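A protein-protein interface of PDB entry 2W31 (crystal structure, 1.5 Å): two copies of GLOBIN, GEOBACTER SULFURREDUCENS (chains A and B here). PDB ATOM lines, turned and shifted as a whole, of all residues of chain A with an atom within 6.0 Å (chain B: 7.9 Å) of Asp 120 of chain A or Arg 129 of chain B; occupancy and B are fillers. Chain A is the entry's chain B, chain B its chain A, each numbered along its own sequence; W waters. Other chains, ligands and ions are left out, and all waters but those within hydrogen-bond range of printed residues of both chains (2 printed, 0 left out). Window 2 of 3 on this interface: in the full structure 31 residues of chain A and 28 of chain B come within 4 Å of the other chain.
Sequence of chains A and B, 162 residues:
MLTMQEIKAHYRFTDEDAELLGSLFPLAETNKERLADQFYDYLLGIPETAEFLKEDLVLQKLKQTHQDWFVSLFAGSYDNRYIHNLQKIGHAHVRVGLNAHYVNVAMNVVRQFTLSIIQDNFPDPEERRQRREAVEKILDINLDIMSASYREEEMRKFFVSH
Among the printed residues, pairs that only touch across the chains: Gln 112 of chain A with Glu 136 of chain B, Leu 115 of chain A with Arg 132 of chain B, Leu 115 of chain A with Glu 136 of chain B, Ser 116 of chain A with Arg 132 of chain B and Gln 119 of chain A with Arg 129 of chain B.
The side-chain amide nitrogen (NE2) of Gln 112 of chain A is in hydrogen-bond range of the backbone carbonyl oxygen (O) of Glu 133 of chain B (3.0 Å). The guanidinium group of Arg 129 of chain B is in hydrogen-bond range of the side-chain hydroxyl of Ser 116 of chain A (3.0 Å). NH2 of Arg 129 of chain B is in salt-bridge range of OD1 of Asp 120 of chain A, at 2.9 Å. NH1 of Arg 132 of chain B lies within hydrogen-bond range of OE1 of Gln 119 of chain A. The side-chain amide nitrogen of Gln 119 of chain A sits at hydrogen-bond distance from the backbone carbonyl oxygen of Pro 125 of chain B (2.7 Å).
The backbone carbonyl oxygen (O) of Gln 112 of chain A is in hydrogen-bond range of the side-chain hydroxyl (OG) of Ser 116 of chain A, 3.4 Å away. The guanidinium group (NH2) of Arg 129 of chain B is in salt-bridge range of the side-chain carboxylate (OE2) of Glu 126 of chain B, 2.9 Å away.
Of the printed residues of chain B, Gln 112 of chain A touches Glu 133 and Glu 136. Of the printed residues of chain B, Gln 119 of chain A touches Pro 125 (2.7 Å), Arg 129 (3.6 Å) and Arg 132 (2.8 Å). Asp 120 of chain A touches just one residue of chain B: Arg 129 (2.9 Å). Of the printed residues of chain A, Arg 129 of chain B touches Ser 116 (3.0 Å), Gln 119 (3.6 Å) and Asp 120 (2.9 Å). Of the printed residues of chain A, Arg 132 of chain B touches Leu 115, Ser 116 and Gln 119. Of the printed residues of chain A, Glu 133 of chain B touches Gln 112 (3.0 Å). The nearest residue of chain A that does not touch Arg 129 of chain B is Leu 115 of chain A (5.7 Å). The nearest printed residue of chain B that does not touch Gln 119 of chain A is Arg 128 of chain B (4.1 Å).
Positions printed for both chains: 118 and 122.
Printed residues of chain A that touch a printed residue of chain B: Gln 112, Leu 115, Ser 116, Gln 119 and Asp 120. Hydrophobic or aromatic side chains of chain A within 4 Å of the printed part of chain B: Leu 115. Along chain B the printed residues that touch a printed residue of chain A span positions 125 to 136. Among the printed residues, 10 pairs touch across the chains.
Water W1 lies within hydrogen-bond range of OE2 of Glu 133 of chain B, OG of Ser 116 of chain A and O of Gln 112 of chain A. Water W2 bridges the backbone carbonyl oxygen of Gln 119 of chain A and the guanidinium group of Arg 128 of chain B.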
ATOM      1  N   GLN A 112     -33.431  -3.254  15.988  1.00  0.00           N
ATOM      2  CA  GLN A 112     -32.605  -4.471  16.062  1.00  0.00           C
ATOM      3  C   GLN A 112     -33.183  -5.564  15.143  1.00  0.00           C
ATOM      4  O   GLN A 112     -32.459  -6.284  14.447  1.00  0.00           O
ATOM      5  CB  GLN A 112     -32.528  -4.995  17.511  1.00  0.00           C
ATOM      6  CG  GLN A 112     -32.016  -4.006  18.597  1.00  0.00           C
ATOM      7  CD  GLN A 112     -30.512  -3.729  18.615  1.00  0.00           C
ATOM      8  OE1 GLN A 112     -29.810  -3.936  17.610  1.00  0.00           O
ATOM      9  NE2 GLN A 112     -30.004  -3.213  19.777  1.00  0.00           N
ATOM     10  N   LEU A 115     -32.559  -4.526  11.353  1.00  0.00           N
ATOM     11  CA  LEU A 115     -31.159  -4.664  10.937  1.00  0.00           C
ATOM     12  C   LEU A 115     -30.719  -6.142  10.863  1.00  0.00           C
ATOM     13  O   LEU A 115     -29.820  -6.496  10.068  1.00  0.00           O
ATOM     14  CB  LEU A 115     -30.227  -3.808  11.819  1.00  0.00           C
ATOM     15  CG  LEU A 115     -30.438  -2.294  11.697  1.00  0.00           C
ATOM     16  CD1 LEU A 115     -29.193  -1.653  12.238  1.00  0.00           C
ATOM     17  CD2 LEU A 115     -30.756  -1.721  10.354  1.00  0.00           C
ATOM     18  N   SER A 116     -31.340  -7.004  11.676  1.00  0.00           N
ATOM     19  CA  SER A 116     -31.076  -8.463  11.529  1.00  0.00           C
ATOM     20  C   SER A 116     -31.647  -9.021  10.225  1.00  0.00           C
ATOM     21  O   SER A 116     -31.021  -9.885   9.609  1.00  0.00           O
ATOM     22  CB  SER A 116     -31.568  -9.240  12.753  1.00  0.00           C
ATOM     23  OG  SER A 116     -30.605  -9.089  13.796  1.00  0.00           O
ATOM     24  N   ILE A 117     -32.824  -8.552   9.804  1.00  0.00           N
ATOM     25  CA  ILE A 117     -33.334  -8.936   8.464  1.00  0.00           C
ATOM     26  C   ILE A 117     -32.289  -8.546   7.408  1.00  0.00           C
ATOM     27  O   ILE A 117     -31.971  -9.340   6.513  1.00  0.00           O
ATOM     28  CB  ILE A 117     -34.684  -8.233   8.127  1.00  0.00           C
ATOM     29  CG1 ILE A 117     -35.833  -8.736   8.999  1.00  0.00           C
ATOM     30  CG2 ILE A 117     -35.035  -8.414   6.655  1.00  0.00           C
ATOM     31  CD1 ILE A 117     -37.143  -7.947   8.817  1.00  0.00           C
ATOM     32  N   ILE A 118     -31.720  -7.339   7.491  1.00  0.00           N
ATOM     33  CA  ILE A 118     -30.737  -6.884   6.512  1.00  0.00           C
ATOM     34  C   ILE A 118     -29.483  -7.787   6.538  1.00  0.00           C
ATOM     35  O   ILE A 118     -29.027  -8.266   5.497  1.00  0.00           O
ATOM     36  CB  ILE A 118     -30.368  -5.370   6.746  1.00  0.00           C
ATOM     37  CG1 ILE A 118     -31.605  -4.458   6.584  1.00  0.00           C
ATOM     38  CG2 ILE A 118     -29.144  -4.938   5.888  1.00  0.00           C
ATOM     39  CD1 ILE A 118     -32.439  -4.628   5.320  1.00  0.00           C
ATOM     40  N   GLN A 119     -28.926  -8.008   7.738  1.00  0.00           N
ATOM     41  CA  GLN A 119     -27.727  -8.846   7.823  1.00  0.00           C
ATOM     42  C   GLN A 119     -27.978 -10.259   7.310  1.00  0.00           C
ATOM     43  O   GLN A 119     -27.098 -10.861   6.659  1.00  0.00           O
ATOM     44  CB  GLN A 119     -27.229  -8.899   9.289  1.00  0.00           C
ATOM     45  CG  GLN A 119     -26.164  -9.954   9.569  1.00  0.00           C
ATOM     46  CD  GLN A 119     -25.676  -9.929  11.021  1.00  0.00           C
ATOM     47  OE1 GLN A 119     -26.054  -9.039  11.809  1.00  0.00           O
ATOM     48  NE2 GLN A 119     -24.838 -10.878  11.367  1.00  0.00           N
ATOM     49  N   ASP A 120     -29.150 -10.786   7.623  1.00  0.00           N
ATOM     50  CA  ASP A 120     -29.507 -12.201   7.370  1.00  0.00           C
ATOM     51  C   ASP A 120     -29.865 -12.489   5.907  1.00  0.00           C
ATOM     52  O   ASP A 120     -29.836 -13.660   5.474  1.00  0.00           O
ATOM     53  CB  ASP A 120     -30.614 -12.693   8.319  1.00  0.00           C
ATOM     54  CG  ASP A 120     -30.141 -12.786   9.773  1.00  0.00           C
ATOM     55  OD1 ASP A 120     -28.907 -12.769  10.000  1.00  0.00           O
ATOM     56  OD2 ASP A 120     -31.008 -12.881  10.667  1.00  0.00           O
ATOM     57  N   ASN A 121     -30.169 -11.437   5.152  1.00  0.00           N
ATOM     58  CA  ASN A 121     -30.641 -11.598   3.770  1.00  0.00           C
ATOM     59  C   ASN A 121     -29.729 -10.972   2.710  1.00  0.00           C
ATOM     60  O   ASN A 121     -29.969 -11.203   1.509  1.00  0.00           O
ATOM     61  CB  ASN A 121     -32.083 -11.036   3.639  1.00  0.00           C
ATOM     62  CG  ASN A 121     -33.108 -11.850   4.438  1.00  0.00           C
ATOM     63  OD1 ASN A 121     -33.475 -11.550   5.585  1.00  0.00           O
ATOM     64  ND2 ASN A 121     -33.516 -12.958   3.843  1.00  0.00           N
ATOM     65  N   PHE A 122     -28.729 -10.179   3.090  1.00  0.00           N
ATOM     66  CA  PHE A 122     -27.852  -9.481   2.124  1.00  0.00           C
ATOM     67  C   PHE A 122     -26.356  -9.739   2.394  1.00  0.00           C
ATOM     68  O   PHE A 122     -25.701  -8.944   3.095  1.00  0.00           O
ATOM     69  CB  PHE A 122     -28.180  -7.973   1.998  1.00  0.00           C
ATOM     70  CG  PHE A 122     -29.606  -7.711   1.556  1.00  0.00           C
ATOM     71  CD1 PHE A 122     -29.948  -7.615   0.204  1.00  0.00           C
ATOM     72  CD2 PHE A 122     -30.638  -7.590   2.517  1.00  0.00           C
ATOM     73  CE1 PHE A 122     -31.278  -7.410  -0.169  1.00  0.00           C
ATOM     74  CE2 PHE A 122     -31.967  -7.396   2.134  1.00  0.00           C
ATOM     75  CZ  PHE A 122     -32.284  -7.286   0.777  1.00  0.00           C
ATOM     76  N   PRO A 123     -25.799 -10.825   1.777  1.00  0.00           N
ATOM     77  CA  PRO A 123     -24.365 -11.150   1.863  1.00  0.00           C
ATOM     78  C   PRO A 123     -23.438 -10.054   1.333  1.00  0.00           C
ATOM     79  O   PRO A 123     -22.346  -9.865   1.894  1.00  0.00           O
ATOM     80  CB  PRO A 123     -24.225 -12.410   0.999  1.00  0.00           C
ATOM     81  CG  PRO A 123     -25.563 -12.976   0.848  1.00  0.00           C
ATOM     82  CD  PRO A 123     -26.536 -11.808   0.966  1.00  0.00           C
ATOM     83  N   ASP B  17     -23.224  -6.454  27.038  1.00  0.00           N
ATOM     84  CA  ASP B  17     -23.181  -5.300  26.157  1.00  0.00           C
ATOM     85  C   ASP B  17     -22.062  -4.335  26.586  1.00  0.00           C
ATOM     86  O   ASP B  17     -21.364  -3.780  25.761  1.00  0.00           O
ATOM     87  CB  ASP B  17     -24.502  -4.552  26.162  1.00  0.00           C
ATOM     88  CG  ASP B  17     -25.628  -5.369  25.581  1.00  0.00           C
ATOM     89  OD1 ASP B  17     -25.620  -5.603  24.362  1.00  0.00           O
ATOM     90  OD2 ASP B  17     -26.536  -5.749  26.343  1.00  0.00           O
ATOM     91  N   LEU B  20     -18.802  -5.636  25.399  1.00  0.00           N
ATOM     92  CA  LEU B  20     -18.612  -5.494  23.967  1.00  0.00           C
ATOM     93  C   LEU B  20     -18.273  -4.058  23.594  1.00  0.00           C
ATOM     94  O   LEU B  20     -17.398  -3.817  22.727  1.00  0.00           O
ATOM     95  CB  LEU B  20     -19.849  -5.976  23.212  1.00  0.00           C
ATOM     96  CG  LEU B  20     -20.088  -7.479  23.252  1.00  0.00           C
ATOM     97  CD1 LEU B  20     -21.568  -7.798  22.905  1.00  0.00           C
ATOM     98  CD2 LEU B  20     -19.067  -8.151  22.318  1.00  0.00           C
ATOM     99  N   ILE B 118     -18.158  -1.074  12.427  1.00  0.00           N
ATOM    100  CA  ILE B 118     -18.419  -2.458  12.785  1.00  0.00           C
ATOM    101  C   ILE B 118     -18.446  -3.337  11.542  1.00  0.00           C
ATOM    102  O   ILE B 118     -17.816  -4.413  11.531  1.00  0.00           O
ATOM    103  CB  ILE B 118     -19.726  -2.581  13.592  1.00  0.00           C
ATOM    104  CG1 ILE B 118     -19.566  -1.896  14.960  1.00  0.00           C
ATOM    105  CG2 ILE B 118     -20.115  -4.064  13.732  1.00  0.00           C
ATOM    106  CD1 ILE B 118     -20.856  -1.873  15.768  1.00  0.00           C
ATOM    107  N   PHE B 122     -15.436  -6.445  11.364  1.00  0.00           N
ATOM    108  CA  PHE B 122     -15.928  -7.708  11.923  1.00  0.00           C
ATOM    109  C   PHE B 122     -16.620  -8.564  10.845  1.00  0.00           C
ATOM    110  O   PHE B 122     -17.847  -8.450  10.634  1.00  0.00           O
ATOM    111  CB  PHE B 122     -16.830  -7.439  13.151  1.00  0.00           C
ATOM    112  CG  PHE B 122     -16.094  -6.772  14.272  1.00  0.00           C
ATOM    113  CD1 PHE B 122     -15.359  -7.541  15.165  1.00  0.00           C
ATOM    114  CD2 PHE B 122     -16.086  -5.378  14.394  1.00  0.00           C
ATOM    115  CE1 PHE B 122     -14.629  -6.927  16.182  1.00  0.00           C
ATOM    116  CE2 PHE B 122     -15.362  -4.761  15.386  1.00  0.00           C
ATOM    117  CZ  PHE B 122     -14.631  -5.528  16.286  1.00  0.00           C
ATOM    118  N   ASP B 124     -17.025 -11.808  10.866  1.00  0.00           N
ATOM    119  CA  ASP B 124     -17.850 -12.865  11.449  1.00  0.00           C
ATOM    120  C   ASP B 124     -19.236 -12.341  11.831  1.00  0.00           C
ATOM    121  O   ASP B 124     -19.320 -11.387  12.674  1.00  0.00           O
ATOM    122  CB  ASP B 124     -17.242 -13.455  12.700  1.00  0.00           C
ATOM    123  CG  ASP B 124     -18.104 -14.555  13.274  1.00  0.00           C
ATOM    124  OD1 ASP B 124     -18.130 -15.669  12.669  1.00  0.00           O
ATOM    125  OD2 ASP B 124     -18.770 -14.336  14.309  1.00  0.00           O
ATOM    126  N   PRO B 125     -20.316 -12.974  11.289  1.00  0.00           N
ATOM    127  CA  PRO B 125     -21.721 -12.507  11.440  1.00  0.00           C
ATOM    128  C   PRO B 125     -22.219 -12.301  12.873  1.00  0.00           C
ATOM    129  O   PRO B 125     -22.909 -11.321  13.134  1.00  0.00           O
ATOM    130  CB  PRO B 125     -22.544 -13.612  10.743  1.00  0.00           C
ATOM    131  CG  PRO B 125     -21.579 -14.255   9.799  1.00  0.00           C
ATOM    132  CD  PRO B 125     -20.239 -14.202  10.457  1.00  0.00           C
ATOM    133  N   GLU B 126     -21.908 -13.184  13.810  1.00  0.00           N
ATOM    134  CA  GLU B 126     -22.467 -13.115  15.131  1.00  0.00           C
ATOM    135  C   GLU B 126     -21.621 -12.147  15.934  1.00  0.00           C
ATOM    136  O   GLU B 126     -22.159 -11.467  16.803  1.00  0.00           O
ATOM    137  CB  GLU B 126     -22.539 -14.509  15.763  1.00  0.00           C
ATOM    138  CG  GLU B 126     -23.619 -15.449  15.139  1.00  0.00           C
ATOM    139  CD  GLU B 126     -24.965 -14.754  14.797  1.00  0.00           C
ATOM    140  OE1 GLU B 126     -25.497 -14.049  15.689  1.00  0.00           O
ATOM    141  OE2 GLU B 126     -25.495 -14.936  13.657  1.00  0.00           O
ATOM    142  N   GLU B 127     -20.318 -12.051  15.630  1.00  0.00           N
ATOM    143  CA  GLU B 127     -19.506 -11.009  16.287  1.00  0.00           C
ATOM    144  C   GLU B 127     -20.079  -9.648  15.892  1.00  0.00           C
ATOM    145  O   GLU B 127     -20.257  -8.743  16.732  1.00  0.00           O
ATOM    146  CB  GLU B 127     -18.020 -11.081  15.895  1.00  0.00           C
ATOM    147  CG  GLU B 127     -17.246 -12.214  16.570  1.00  0.00           C
ATOM    148  CD  GLU B 127     -15.734 -12.157  16.311  1.00  0.00           C
ATOM    149  OE1 GLU B 127     -15.240 -11.226  15.633  1.00  0.00           O
ATOM    150  OE2 GLU B 127     -15.016 -13.069  16.806  1.00  0.00           O
ATOM    151  N   ARG B 128     -20.361  -9.499  14.602  1.00  0.00           N
ATOM    152  CA  ARG B 128     -20.897  -8.245  14.066  1.00  0.00           C
ATOM    153  C   ARG B 128     -22.278  -7.951  14.685  1.00  0.00           C
ATOM    154  O   ARG B 128     -22.541  -6.812  15.131  1.00  0.00           O
ATOM    155  CB  ARG B 128     -20.963  -8.374  12.524  1.00  0.00           C
ATOM    156  CG  ARG B 128     -21.171  -7.103  11.819  1.00  0.00           C
ATOM    157  CD  ARG B 128     -20.816  -7.178  10.341  1.00  0.00           C
ATOM    158  NE  ARG B 128     -21.672  -8.110   9.622  1.00  0.00           N
ATOM    159  CZ  ARG B 128     -21.240  -9.236   9.069  1.00  0.00           C
ATOM    160  NH1 ARG B 128     -19.963  -9.575   9.178  1.00  0.00           N
ATOM    161  NH2 ARG B 128     -22.084 -10.032   8.432  1.00  0.00           N
ATOM    162  N   ARG B 129     -23.146  -8.974  14.743  1.00  0.00           N
ATOM    163  CA  ARG B 129     -24.497  -8.775  15.267  1.00  0.00           C
ATOM    164  C   ARG B 129     -24.448  -8.297  16.726  1.00  0.00           C
ATOM    165  O   ARG B 129     -25.106  -7.316  17.121  1.00  0.00           O
ATOM    166  CB  ARG B 129     -25.341 -10.042  15.168  1.00  0.00           C
ATOM    167  CG  ARG B 129     -26.837  -9.764  15.428  1.00  0.00           C
ATOM    168  CD  ARG B 129     -27.689 -11.052  15.576  1.00  0.00           C
ATOM    169  NE  ARG B 129     -27.342 -12.066  14.560  1.00  0.00           N
ATOM    170  CZ  ARG B 129     -27.892 -12.186  13.341  1.00  0.00           C
ATOM    171  NH1 ARG B 129     -28.885 -11.381  12.919  1.00  0.00           N
ATOM    172  NH2 ARG B 129     -27.477 -13.161  12.540  1.00  0.00           N
ATOM    173  N   GLN B 130     -23.627  -8.968  17.524  1.00  0.00           N
ATOM    174  CA  GLN B 130     -23.528  -8.633  18.937  1.00  0.00           C
ATOM    175  C   GLN B 130     -22.991  -7.221  19.177  1.00  0.00           C
ATOM    176  O   GLN B 130     -23.525  -6.508  20.050  1.00  0.00           O
ATOM    177  CB  GLN B 130     -22.673  -9.676  19.673  1.00  0.00           C
ATOM    178  CG  GLN B 130     -23.376 -11.013  19.903  1.00  0.00           C
ATOM    179  CD  GLN B 130     -22.486 -11.980  20.706  1.00  0.00           C
ATOM    180  OE1 GLN B 130     -21.484 -11.568  21.289  1.00  0.00           O
ATOM    181  NE2 GLN B 130     -22.856 -13.277  20.731  1.00  0.00           N
ATOM    182  N   ARG B 131     -21.982  -6.812  18.409  1.00  0.00           N
ATOM    183  CA  ARG B 131     -21.410  -5.456  18.530  1.00  0.00           C
ATOM    184  C   ARG B 131     -22.388  -4.385  18.034  1.00  0.00           C
ATOM    185  O   ARG B 131     -22.558  -3.348  18.699  1.00  0.00           O
ATOM    186  CB  ARG B 131     -20.057  -5.363  17.814  1.00  0.00           C
ATOM    187  CG  ARG B 131     -18.965  -6.096  18.606  1.00  0.00           C
ATOM    188  CD  ARG B 131     -17.791  -6.583  17.749  1.00  0.00           C
ATOM    189  NE  ARG B 131     -16.818  -7.284  18.598  1.00  0.00           N
ATOM    190  CZ  ARG B 131     -16.981  -8.505  19.099  1.00  0.00           C
ATOM    191  NH1 ARG B 131     -18.074  -9.213  18.836  1.00  0.00           N
ATOM    192  NH2 ARG B 131     -16.036  -9.025  19.900  1.00  0.00           N
ATOM    193  N   ARG B 132     -23.080  -4.664  16.918  1.00  0.00           N
ATOM    194  CA  ARG B 132     -24.096  -3.736  16.437  1.00  0.00           C
ATOM    195  C   ARG B 132     -25.206  -3.595  17.483  1.00  0.00           C
ATOM    196  O   ARG B 132     -25.681  -2.460  17.740  1.00  0.00           O
ATOM    197  CB  ARG B 132     -24.673  -4.198  15.090  1.00  0.00           C
ATOM    198  CG  ARG B 132     -25.529  -3.134  14.394  1.00  0.00           C
ATOM    199  CD  ARG B 132     -26.173  -3.646  13.119  1.00  0.00           C
ATOM    200  NE  ARG B 132     -27.013  -4.830  13.350  1.00  0.00           N
ATOM    201  CZ  ARG B 132     -26.780  -6.043  12.845  1.00  0.00           C
ATOM    202  NH1 ARG B 132     -25.739  -6.261  12.061  1.00  0.00           N
ATOM    203  NH2 ARG B 132     -27.603  -7.044  13.125  1.00  0.00           N
ATOM    204  N   GLU B 133     -25.660  -4.726  18.064  1.00  0.00           N
ATOM    205  CA  GLU B 133     -26.743  -4.619  19.043  1.00  0.00           C
ATOM    206  C   GLU B 133     -26.342  -3.770  20.267  1.00  0.00           C
ATOM    207  O   GLU B 133     -27.135  -2.963  20.743  1.00  0.00           O
ATOM    208  CB  GLU B 133     -27.241  -6.005  19.491  1.00  0.00           C
ATOM    209  CG  GLU B 133     -28.064  -6.759  18.391  1.00  0.00           C
ATOM    210  CD  GLU B 133     -28.345  -8.226  18.715  1.00  0.00           C
ATOM    211  OE1 GLU B 133     -27.624  -8.811  19.548  1.00  0.00           O
ATOM    212  OE2 GLU B 133     -29.232  -8.813  18.065  1.00  0.00           O
ATOM    213  N   ALA B 134     -25.092  -3.920  20.746  1.00  0.00           N
ATOM    214  CA  ALA B 134     -24.625  -3.156  21.910  1.00  0.00           C
ATOM    215  C   ALA B 134     -24.578  -1.648  21.563  1.00  0.00           C
ATOM    216  O   ALA B 134     -24.976  -0.799  22.376  1.00  0.00           O
ATOM    217  CB  ALA B 134     -23.216  -3.643  22.344  1.00  0.00           C
ATOM    218  N   VAL B 135     -24.035  -1.315  20.382  1.00  0.00           N
ATOM    219  CA  VAL B 135     -23.906   0.098  19.967  1.00  0.00           C
ATOM    220  C   VAL B 135     -25.300   0.711  19.779  1.00  0.00           C
ATOM    221  O   VAL B 135     -25.553   1.842  20.222  1.00  0.00           O
ATOM    222  CB  VAL B 135     -23.108   0.220  18.656  1.00  0.00           C
ATOM    223  CG1 VAL B 135     -23.335   1.567  17.977  1.00  0.00           C
ATOM    224  CG2 VAL B 135     -21.629  -0.036  18.949  1.00  0.00           C
ATOM    225  N   GLU B 136     -26.215  -0.024  19.137  1.00  0.00           N
ATOM    226  CA  GLU B 136     -27.574   0.548  18.991  1.00  0.00           C
ATOM    227  C   GLU B 136     -28.244   0.819  20.331  1.00  0.00           C
ATOM    228  O   GLU B 136     -28.936   1.844  20.480  1.00  0.00           O
ATOM    229  CB  GLU B 136     -28.464  -0.315  18.115  1.00  0.00           C
ATOM    230  CG  GLU B 136     -27.992  -0.470  16.683  1.00  0.00           C
ATOM    231  CD  GLU B 136     -28.359   0.646  15.765  1.00  0.00           C
ATOM    232  OE1 GLU B 136     -28.233   1.842  16.098  1.00  0.00           O
ATOM    233  OE2 GLU B 136     -28.722   0.314  14.604  1.00  0.00           O
HETATM  234  O   HOH W   1     -30.980  -8.225  16.262  1.00  0.00           O
HETATM  235  O   HOH W   2     -24.429 -10.589   6.645  1.00  0.00           O
